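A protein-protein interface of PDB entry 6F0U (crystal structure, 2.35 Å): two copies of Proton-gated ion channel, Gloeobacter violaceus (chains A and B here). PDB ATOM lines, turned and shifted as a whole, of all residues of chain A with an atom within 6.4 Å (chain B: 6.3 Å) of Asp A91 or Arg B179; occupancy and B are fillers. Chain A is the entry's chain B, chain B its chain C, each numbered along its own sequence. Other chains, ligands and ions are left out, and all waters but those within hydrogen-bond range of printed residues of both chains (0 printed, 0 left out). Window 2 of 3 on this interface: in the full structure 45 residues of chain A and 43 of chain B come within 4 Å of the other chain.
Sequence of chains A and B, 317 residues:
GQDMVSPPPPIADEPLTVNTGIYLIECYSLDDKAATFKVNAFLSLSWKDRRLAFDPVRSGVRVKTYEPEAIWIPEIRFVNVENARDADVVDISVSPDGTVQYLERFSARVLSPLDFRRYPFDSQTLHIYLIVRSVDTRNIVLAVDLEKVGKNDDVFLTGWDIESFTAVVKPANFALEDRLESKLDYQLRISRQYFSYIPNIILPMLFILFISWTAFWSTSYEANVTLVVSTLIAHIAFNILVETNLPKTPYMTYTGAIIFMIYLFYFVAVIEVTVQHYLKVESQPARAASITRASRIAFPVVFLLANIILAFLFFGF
OD2 of Asp A91 is in salt-bridge range of NH1 of Arg B179 (3.7 Å). OE1 of Glu B75 sits close to O of Val A90 (2.6 Å).
The side-chain carboxylate of Asp A91 sits at hydrogen-bond distance from the side-chain hydroxyl of Ser A93 (3.0 Å). The guanidinium group (NH1) of Arg B133 is in salt-bridge range of the side-chain carboxylate (OE1) of Glu B181, at 2.7 Å. O of Asp A91 sits at hydrogen-bond distance from N of Leu A103. NH1 of Arg B133 lies within hydrogen-bond range of O of Leu B176 (2.7 Å). OD2 of Asp B136 is in salt-bridge range of NH2 of Arg B179 (3.2 Å). NH2 of Arg B133 lies within hydrogen-bond range of O of Glu B177.
CG2 of Val A63 touches CB of Asp B136 (3.6 Å). Leu A103 touches Arg B133.
Of chain A, only Asp A91 comes within 4 Å of Arg B179. Of the printed residues of chain A, Asp B136 touches Val A63 (3.6 Å). Printed residues of chain A within 4 Å of Arg B133: Leu A103. Printed residues of chain B within 4 Å of Leu A103: Arg B133 (3.7 Å). Of the printed residues of chain B, Val A90 touches Glu B75 (2.6 Å). Of the printed residues of chain B, Val A63 touches Asp B136. Glu A104 touches none of the printed residues of chain B. The nearest residue of chain B that does not touch Asp A91 is Glu B75 (4.7 Å). The nearest residue of chain A that does not touch Arg B179 is Ser A93 (4.3 Å). The nearest printed residue of chain A that does not touch Asp B136 is Ser A93 (5.2 Å).
Hydrophobic or aromatic side chains of chain A that line the printed part of chain B: Val A63, Val A90 and Leu A103. Of the 13 printed residues of chain B, 4 touch a printed residue of chain A. Along chain B the printed residues that touch a printed residue of chain A span positions 75 to 179. Among the printed residues, 4 pairs touch across the chains. Among the printed residues, Asp or Glu carboxylates within 4 Å of a Lys or Arg side-chain nitrogen of the other chain: Asp A91 with Arg B179 (3.7 Å).
No position is printed for both chains. Of the 4 pairs that touch across the chains among the printed residues, none has its exchanged pair printed and touching as well.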
ATOM      1  N   VAL A  63       2.089   0.377 -15.798  1.00  0.00           N
ATOM      2  CA  VAL A  63       1.903  -0.632 -16.840  1.00  0.00           C
ATOM      3  C   VAL A  63       1.985  -1.993 -16.181  1.00  0.00           C
ATOM      4  O   VAL A  63       2.742  -2.176 -15.237  1.00  0.00           O
ATOM      5  CB  VAL A  63       2.946  -0.521 -17.983  1.00  0.00           C
ATOM      6  CG1 VAL A  63       2.687   0.695 -18.869  1.00  0.00           C
ATOM      7  CG2 VAL A  63       4.361  -0.500 -17.435  1.00  0.00           C
ATOM      8  N   THR A  65       2.594  -6.263 -16.426  1.00  0.00           N
ATOM      9  CA  THR A  65       3.242  -7.304 -17.184  1.00  0.00           C
ATOM     10  C   THR A  65       2.441  -8.566 -16.992  1.00  0.00           C
ATOM     11  O   THR A  65       2.317  -9.049 -15.870  1.00  0.00           O
ATOM     12  CB  THR A  65       4.695  -7.483 -16.758  1.00  0.00           C
ATOM     13  OG1 THR A  65       5.491  -6.499 -17.401  1.00  0.00           O
ATOM     14  CG2 THR A  65       5.229  -8.852 -17.118  1.00  0.00           C
ATOM     15  N   TYR A  66       1.891  -9.116 -18.083  1.00  0.00           N
ATOM     16  CA  TYR A  66       1.138 -10.359 -18.008  1.00  0.00           C
ATOM     17  C   TYR A  66       1.932 -11.482 -18.632  1.00  0.00           C
ATOM     18  O   TYR A  66       2.824 -11.247 -19.451  1.00  0.00           O
ATOM     19  CB  TYR A  66      -0.206 -10.250 -18.715  1.00  0.00           C
ATOM     20  CG  TYR A  66      -1.235  -9.399 -18.007  1.00  0.00           C
ATOM     21  CD1 TYR A  66      -1.335  -8.037 -18.261  1.00  0.00           C
ATOM     22  CD2 TYR A  66      -2.192  -9.975 -17.176  1.00  0.00           C
ATOM     23  CE1 TYR A  66      -2.340  -7.258 -17.678  1.00  0.00           C
ATOM     24  CE2 TYR A  66      -3.205  -9.209 -16.593  1.00  0.00           C
ATOM     25  CZ  TYR A  66      -3.280  -7.851 -16.848  1.00  0.00           C
ATOM     26  OH  TYR A  66      -4.282  -7.092 -16.276  1.00  0.00           O
ATOM     27  N   ASP A  88       9.732 -17.349 -28.580  1.00  0.00           N
ATOM     28  CA  ASP A  88       9.939 -17.111 -27.166  1.00  0.00           C
ATOM     29  C   ASP A  88       9.469 -15.700 -26.819  1.00  0.00           C
ATOM     30  O   ASP A  88       9.998 -14.716 -27.349  1.00  0.00           O
ATOM     31  CB  ASP A  88      11.393 -17.401 -26.751  1.00  0.00           C
ATOM     32  CG  ASP A  88      11.746 -18.883 -26.791  1.00  0.00           C
ATOM     33  OD1 ASP A  88      11.306 -19.627 -25.877  1.00  0.00           O
ATOM     34  OD2 ASP A  88      12.445 -19.303 -27.747  1.00  0.00           O
ATOM     35  N   VAL A  89       8.416 -15.609 -25.977  1.00  0.00           N
ATOM     36  CA  VAL A  89       7.832 -14.331 -25.558  1.00  0.00           C
ATOM     37  C   VAL A  89       8.876 -13.543 -24.742  1.00  0.00           C
ATOM     38  O   VAL A  89       9.521 -14.096 -23.836  1.00  0.00           O
ATOM     39  CB  VAL A  89       6.474 -14.491 -24.825  1.00  0.00           C
ATOM     40  CG1 VAL A  89       5.916 -13.149 -24.385  1.00  0.00           C
ATOM     41  CG2 VAL A  89       5.457 -15.206 -25.701  1.00  0.00           C
ATOM     42  N   VAL A  90       9.099 -12.286 -25.142  1.00  0.00           N
ATOM     43  CA  VAL A  90      10.035 -11.378 -24.505  1.00  0.00           C
ATOM     44  C   VAL A  90       9.284 -10.484 -23.527  1.00  0.00           C
ATOM     45  O   VAL A  90       9.695 -10.350 -22.372  1.00  0.00           O
ATOM     46  CB  VAL A  90      10.834 -10.566 -25.560  1.00  0.00           C
ATOM     47  CG1 VAL A  90      11.593  -9.401 -24.918  1.00  0.00           C
ATOM     48  CG2 VAL A  90      11.789 -11.473 -26.338  1.00  0.00           C
ATOM     49  N   ASP A  91       8.169  -9.875 -23.977  1.00  0.00           N
ATOM     50  CA  ASP A  91       7.414  -8.975 -23.142  1.00  0.00           C
ATOM     51  C   ASP A  91       5.978  -8.814 -23.570  1.00  0.00           C
ATOM     52  O   ASP A  91       5.683  -8.806 -24.762  1.00  0.00           O
ATOM     53  CB  ASP A  91       8.109  -7.603 -23.107  1.00  0.00           C
ATOM     54  CG  ASP A  91       7.590  -6.665 -22.031  1.00  0.00           C
ATOM     55  OD1 ASP A  91       7.440  -7.115 -20.866  1.00  0.00           O
ATOM     56  OD2 ASP A  91       7.338  -5.487 -22.348  1.00  0.00           O
ATOM     57  N   ILE A  92       5.086  -8.670 -22.569  1.00  0.00           N
ATOM     58  CA  ILE A  92       3.674  -8.376 -22.715  1.00  0.00           C
ATOM     59  C   ILE A  92       3.404  -7.243 -21.732  1.00  0.00           C
ATOM     60  O   ILE A  92       3.532  -7.434 -20.523  1.00  0.00           O
ATOM     61  CB  ILE A  92       2.736  -9.595 -22.511  1.00  0.00           C
ATOM     62  CG1 ILE A  92       3.070 -10.734 -23.503  1.00  0.00           C
ATOM     63  CG2 ILE A  92       1.266  -9.158 -22.641  1.00  0.00           C
ATOM     64  CD1 ILE A  92       2.406 -12.050 -23.254  1.00  0.00           C
ATOM     65  N   SER A  93       3.092  -6.051 -22.266  1.00  0.00           N
ATOM     66  CA  SER A  93       2.823  -4.847 -21.484  1.00  0.00           C
ATOM     67  C   SER A  93       1.448  -4.284 -21.788  1.00  0.00           C
ATOM     68  O   SER A  93       1.113  -4.077 -22.946  1.00  0.00           O
ATOM     69  CB  SER A  93       3.903  -3.798 -21.725  1.00  0.00           C
ATOM     70  OG  SER A  93       5.043  -4.112 -20.943  1.00  0.00           O
ATOM     71  N   GLN A 101       0.864  -4.541 -25.636  1.00  0.00           N
ATOM     72  CA  GLN A 101       2.079  -4.465 -26.429  1.00  0.00           C
ATOM     73  C   GLN A 101       2.834  -5.749 -26.175  1.00  0.00           C
ATOM     74  O   GLN A 101       3.309  -6.000 -25.061  1.00  0.00           O
ATOM     75  CB  GLN A 101       2.904  -3.210 -26.109  1.00  0.00           C
ATOM     76  CG  GLN A 101       2.270  -1.932 -26.668  1.00  0.00           C
ATOM     77  CD  GLN A 101       3.306  -0.966 -27.211  1.00  0.00           C
ATOM     78  OE1 GLN A 101       4.260  -0.584 -26.523  1.00  0.00           O
ATOM     79  NE2 GLN A 101       3.135  -0.539 -28.463  1.00  0.00           N
ATOM     80  N   TYR A 102       2.825  -6.617 -27.200  1.00  0.00           N
ATOM     81  CA  TYR A 102       3.419  -7.946 -27.209  1.00  0.00           C
ATOM     82  C   TYR A 102       4.689  -7.938 -28.033  1.00  0.00           C
ATOM     83  O   TYR A 102       4.738  -7.330 -29.113  1.00  0.00           O
ATOM     84  CB  TYR A 102       2.391  -8.951 -27.775  1.00  0.00           C
ATOM     85  CG  TYR A 102       2.891 -10.357 -27.992  1.00  0.00           C
ATOM     86  CD1 TYR A 102       3.569 -10.703 -29.161  1.00  0.00           C
ATOM     87  CD2 TYR A 102       2.600 -11.371 -27.083  1.00  0.00           C
ATOM     88  CE1 TYR A 102       3.990 -12.007 -29.392  1.00  0.00           C
ATOM     89  CE2 TYR A 102       3.041 -12.678 -27.294  1.00  0.00           C
ATOM     90  CZ  TYR A 102       3.729 -12.990 -28.454  1.00  0.00           C
ATOM     91  OH  TYR A 102       4.151 -14.272 -28.658  1.00  0.00           O
ATOM     92  N   LEU A 103       5.714  -8.653 -27.532  1.00  0.00           N
ATOM     93  CA  LEU A 103       6.976  -8.831 -28.225  1.00  0.00           C
ATOM     94  C   LEU A 103       7.531 -10.238 -28.029  1.00  0.00           C
ATOM     95  O   LEU A 103       7.661 -10.717 -26.913  1.00  0.00           O
ATOM     96  CB  LEU A 103       8.017  -7.771 -27.825  1.00  0.00           C
ATOM     97  CG  LEU A 103       9.330  -7.801 -28.622  1.00  0.00           C
ATOM     98  CD1 LEU A 103       9.124  -7.366 -30.081  1.00  0.00           C
ATOM     99  CD2 LEU A 103      10.416  -6.974 -27.922  1.00  0.00           C
ATOM    100  N   GLU A 104       7.863 -10.890 -29.123  1.00  0.00           N
ATOM    101  CA  GLU A 104       8.469 -12.216 -29.104  1.00  0.00           C
ATOM    102  C   GLU A 104       9.641 -12.224 -30.020  1.00  0.00           C
ATOM    103  O   GLU A 104       9.707 -11.426 -30.963  1.00  0.00           O
ATOM    104  CB  GLU A 104       7.477 -13.314 -29.535  1.00  0.00           C
ATOM    105  CG  GLU A 104       7.028 -13.236 -30.984  1.00  0.00           C
ATOM    106  CD  GLU A 104       6.341 -14.480 -31.504  1.00  0.00           C
ATOM    107  OE1 GLU A 104       5.195 -14.769 -31.098  1.00  0.00           O
ATOM    108  OE2 GLU A 104       6.953 -15.162 -32.344  1.00  0.00           O
ATOM    109  N   GLU B  75      15.992 -11.109 -18.568  1.00  0.00           N
ATOM    110  CA  GLU B  75      15.856 -11.855 -19.814  1.00  0.00           C
ATOM    111  C   GLU B  75      17.053 -11.516 -20.706  1.00  0.00           C
ATOM    112  O   GLU B  75      17.050 -10.493 -21.411  1.00  0.00           O
ATOM    113  CB  GLU B  75      14.552 -11.504 -20.540  1.00  0.00           C
ATOM    114  CG  GLU B  75      13.266 -11.982 -19.894  1.00  0.00           C
ATOM    115  CD  GLU B  75      12.035 -11.542 -20.665  1.00  0.00           C
ATOM    116  OE1 GLU B  75      12.191 -10.860 -21.704  1.00  0.00           O
ATOM    117  OE2 GLU B  75      10.913 -11.898 -20.242  1.00  0.00           O
ATOM    118  N   ARG B 133      17.245  -6.334 -22.972  1.00  0.00           N
ATOM    119  CA  ARG B 133      16.325  -5.280 -23.349  1.00  0.00           C
ATOM    120  C   ARG B 133      15.746  -4.682 -22.044  1.00  0.00           C
ATOM    121  O   ARG B 133      15.328  -5.430 -21.150  1.00  0.00           O
ATOM    122  CB  ARG B 133      15.235  -5.836 -24.265  1.00  0.00           C
ATOM    123  CG  ARG B 133      14.203  -4.800 -24.686  1.00  0.00           C
ATOM    124  CD  ARG B 133      13.309  -5.326 -25.781  1.00  0.00           C
ATOM    125  NE  ARG B 133      12.311  -4.334 -26.168  1.00  0.00           N
ATOM    126  CZ  ARG B 133      12.487  -3.407 -27.104  1.00  0.00           C
ATOM    127  NH1 ARG B 133      13.649  -3.307 -27.741  1.00  0.00           N
ATOM    128  NH2 ARG B 133      11.504  -2.560 -27.401  1.00  0.00           N
ATOM    129  N   SER B 134      15.766  -3.339 -21.929  1.00  0.00           N
ATOM    130  CA  SER B 134      15.247  -2.614 -20.769  1.00  0.00           C
ATOM    131  C   SER B 134      13.740  -2.792 -20.643  1.00  0.00           C
ATOM    132  O   SER B 134      13.044  -2.998 -21.644  1.00  0.00           O
ATOM    133  CB  SER B 134      15.579  -1.130 -20.863  1.00  0.00           C
ATOM    134  OG  SER B 134      16.932  -0.897 -20.515  1.00  0.00           O
ATOM    135  N   VAL B 135      13.245  -2.719 -19.400  1.00  0.00           N
ATOM    136  CA  VAL B 135      11.821  -2.842 -19.078  1.00  0.00           C
ATOM    137  C   VAL B 135      11.210  -1.464 -18.782  1.00  0.00           C
ATOM    138  O   VAL B 135      11.939  -0.483 -18.604  1.00  0.00           O
ATOM    139  CB  VAL B 135      11.527  -3.886 -17.965  1.00  0.00           C
ATOM    140  CG1 VAL B 135      11.900  -5.297 -18.423  1.00  0.00           C
ATOM    141  CG2 VAL B 135      12.237  -3.539 -16.671  1.00  0.00           C
ATOM    142  N   ASP B 136       9.879  -1.380 -18.735  1.00  0.00           N
ATOM    143  CA  ASP B 136       9.210  -0.101 -18.480  1.00  0.00           C
ATOM    144  C   ASP B 136       9.497   0.468 -17.090  1.00  0.00           C
ATOM    145  O   ASP B 136       9.631   1.688 -16.945  1.00  0.00           O
ATOM    146  CB  ASP B 136       7.701  -0.202 -18.755  1.00  0.00           C
ATOM    147  CG  ASP B 136       7.136   1.046 -19.410  1.00  0.00           C
ATOM    148  OD1 ASP B 136       6.963   2.064 -18.699  1.00  0.00           O
ATOM    149  OD2 ASP B 136       6.879   1.011 -20.643  1.00  0.00           O
ATOM    150  N   PHE B 174      22.119   1.226 -26.838  1.00  0.00           N
ATOM    151  CA  PHE B 174      21.394   1.859 -27.935  1.00  0.00           C
ATOM    152  C   PHE B 174      19.909   1.662 -27.770  1.00  0.00           C
ATOM    153  O   PHE B 174      19.493   0.886 -26.913  1.00  0.00           O
ATOM    154  CB  PHE B 174      21.861   1.269 -29.290  1.00  0.00           C
ATOM    155  CG  PHE B 174      21.632  -0.216 -29.484  1.00  0.00           C
ATOM    156  CD1 PHE B 174      22.487  -1.154 -28.907  1.00  0.00           C
ATOM    157  CD2 PHE B 174      20.598  -0.676 -30.286  1.00  0.00           C
ATOM    158  CE1 PHE B 174      22.284  -2.530 -29.092  1.00  0.00           C
ATOM    159  CE2 PHE B 174      20.389  -2.051 -30.466  1.00  0.00           C
ATOM    160  CZ  PHE B 174      21.236  -2.971 -29.868  1.00  0.00           C
ATOM    161  N   ALA B 175      19.107   2.355 -28.595  1.00  0.00           N
ATOM    162  CA  ALA B 175      17.657   2.249 -28.588  1.00  0.00           C
ATOM    163  C   ALA B 175      17.169   1.409 -29.764  1.00  0.00           C
ATOM    164  O   ALA B 175      17.561   1.656 -30.901  1.00  0.00           O
ATOM    165  CB  ALA B 175      17.035   3.633 -28.647  1.00  0.00           C
ATOM    166  N   LEU B 176      16.338   0.404 -29.481  1.00  0.00           N
ATOM    167  CA  LEU B 176      15.717  -0.442 -30.488  1.00  0.00           C
ATOM    168  C   LEU B 176      14.250  -0.503 -30.131  1.00  0.00           C
ATOM    169  O   LEU B 176      13.905  -0.956 -29.042  1.00  0.00           O
ATOM    170  CB  LEU B 176      16.357  -1.845 -30.534  1.00  0.00           C
ATOM    171  CG  LEU B 176      15.678  -2.948 -31.372  1.00  0.00           C
ATOM    172  CD1 LEU B 176      15.354  -2.486 -32.785  1.00  0.00           C
ATOM    173  CD2 LEU B 176      16.540  -4.177 -31.424  1.00  0.00           C
ATOM    174  N   GLU B 177      13.392  -0.004 -31.029  1.00  0.00           N
ATOM    175  CA  GLU B 177      11.944   0.022 -30.852  1.00  0.00           C
ATOM    176  C   GLU B 177      11.528   0.730 -29.555  1.00  0.00           C
ATOM    177  O   GLU B 177      10.704   0.241 -28.779  1.00  0.00           O
ATOM    178  CB  GLU B 177      11.346  -1.379 -31.006  1.00  0.00           C
ATOM    179  CG  GLU B 177      11.392  -1.873 -32.453  1.00  0.00           C
ATOM    180  CD  GLU B 177      10.504  -3.060 -32.738  1.00  0.00           C
ATOM    181  OE1 GLU B 177      10.624  -3.645 -33.839  1.00  0.00           O
ATOM    182  OE2 GLU B 177       9.685  -3.407 -31.861  1.00  0.00           O
ATOM    183  N   ASP B 178      12.124   1.919 -29.357  1.00  0.00           N
ATOM    184  CA  ASP B 178      11.920   2.867 -28.261  1.00  0.00           C
ATOM    185  C   ASP B 178      12.192   2.294 -26.860  1.00  0.00           C
ATOM    186  O   ASP B 178      11.563   2.688 -25.887  1.00  0.00           O
ATOM    187  CB  ASP B 178      10.539   3.541 -28.338  1.00  0.00           C
ATOM    188  CG  ASP B 178      10.539   4.929 -27.718  1.00  0.00           C
ATOM    189  OD1 ASP B 178      11.640   5.487 -27.498  1.00  0.00           O
ATOM    190  OD2 ASP B 178       9.445   5.452 -27.433  1.00  0.00           O
ATOM    191  N   ARG B 179      13.185   1.418 -26.765  1.00  0.00           N
ATOM    192  CA  ARG B 179      13.666   0.829 -25.513  1.00  0.00           C
ATOM    193  C   ARG B 179      15.158   0.619 -25.593  1.00  0.00           C
ATOM    194  O   ARG B 179      15.681   0.244 -26.648  1.00  0.00           O
ATOM    195  CB  ARG B 179      13.011  -0.517 -25.203  1.00  0.00           C
ATOM    196  CG  ARG B 179      11.585  -0.431 -24.757  1.00  0.00           C
ATOM    197  CD  ARG B 179      11.453  -0.510 -23.260  1.00  0.00           C
ATOM    198  NE  ARG B 179      10.046  -0.458 -22.863  1.00  0.00           N
ATOM    199  CZ  ARG B 179       9.279  -1.529 -22.709  1.00  0.00           C
ATOM    200  NH1 ARG B 179       9.779  -2.745 -22.896  1.00  0.00           N
ATOM    201  NH2 ARG B 179       8.006  -1.396 -22.362  1.00  0.00           N
ATOM    202  N   LEU B 180      15.832   0.834 -24.464  1.00  0.00           N
ATOM    203  CA  LEU B 180      17.264   0.646 -24.325  1.00  0.00           C
ATOM    204  C   LEU B 180      17.606  -0.834 -24.412  1.00  0.00           C
ATOM    205  O   LEU B 180      16.910  -1.684 -23.865  1.00  0.00           O
ATOM    206  CB  LEU B 180      17.764   1.234 -22.991  1.00  0.00           C
ATOM    207  CG  LEU B 180      19.286   1.454 -22.841  1.00  0.00           C
ATOM    208  CD1 LEU B 180      19.561   2.781 -22.160  1.00  0.00           C
ATOM    209  CD2 LEU B 180      19.943   0.333 -22.035  1.00  0.00           C
ATOM    210  N   GLU B 181      18.673  -1.118 -25.142  1.00  0.00           N
ATOM    211  CA  GLU B 181      19.255  -2.430 -25.311  1.00  0.00           C
ATOM    212  C   GLU B 181      20.706  -2.241 -24.904  1.00  0.00           C
ATOM    213  O   GLU B 181      21.290  -1.193 -25.205  1.00  0.00           O
ATOM    214  CB  GLU B 181      19.160  -2.894 -26.779  1.00  0.00           C
ATOM    215  CG  GLU B 181      17.746  -3.115 -27.305  1.00  0.00           C
ATOM    216  CD  GLU B 181      17.193  -4.529 -27.239  1.00  0.00           C
ATOM    217  OE1 GLU B 181      15.993  -4.694 -27.555  1.00  0.00           O
ATOM    218  OE2 GLU B 181      17.945  -5.471 -26.895  1.00  0.00           O
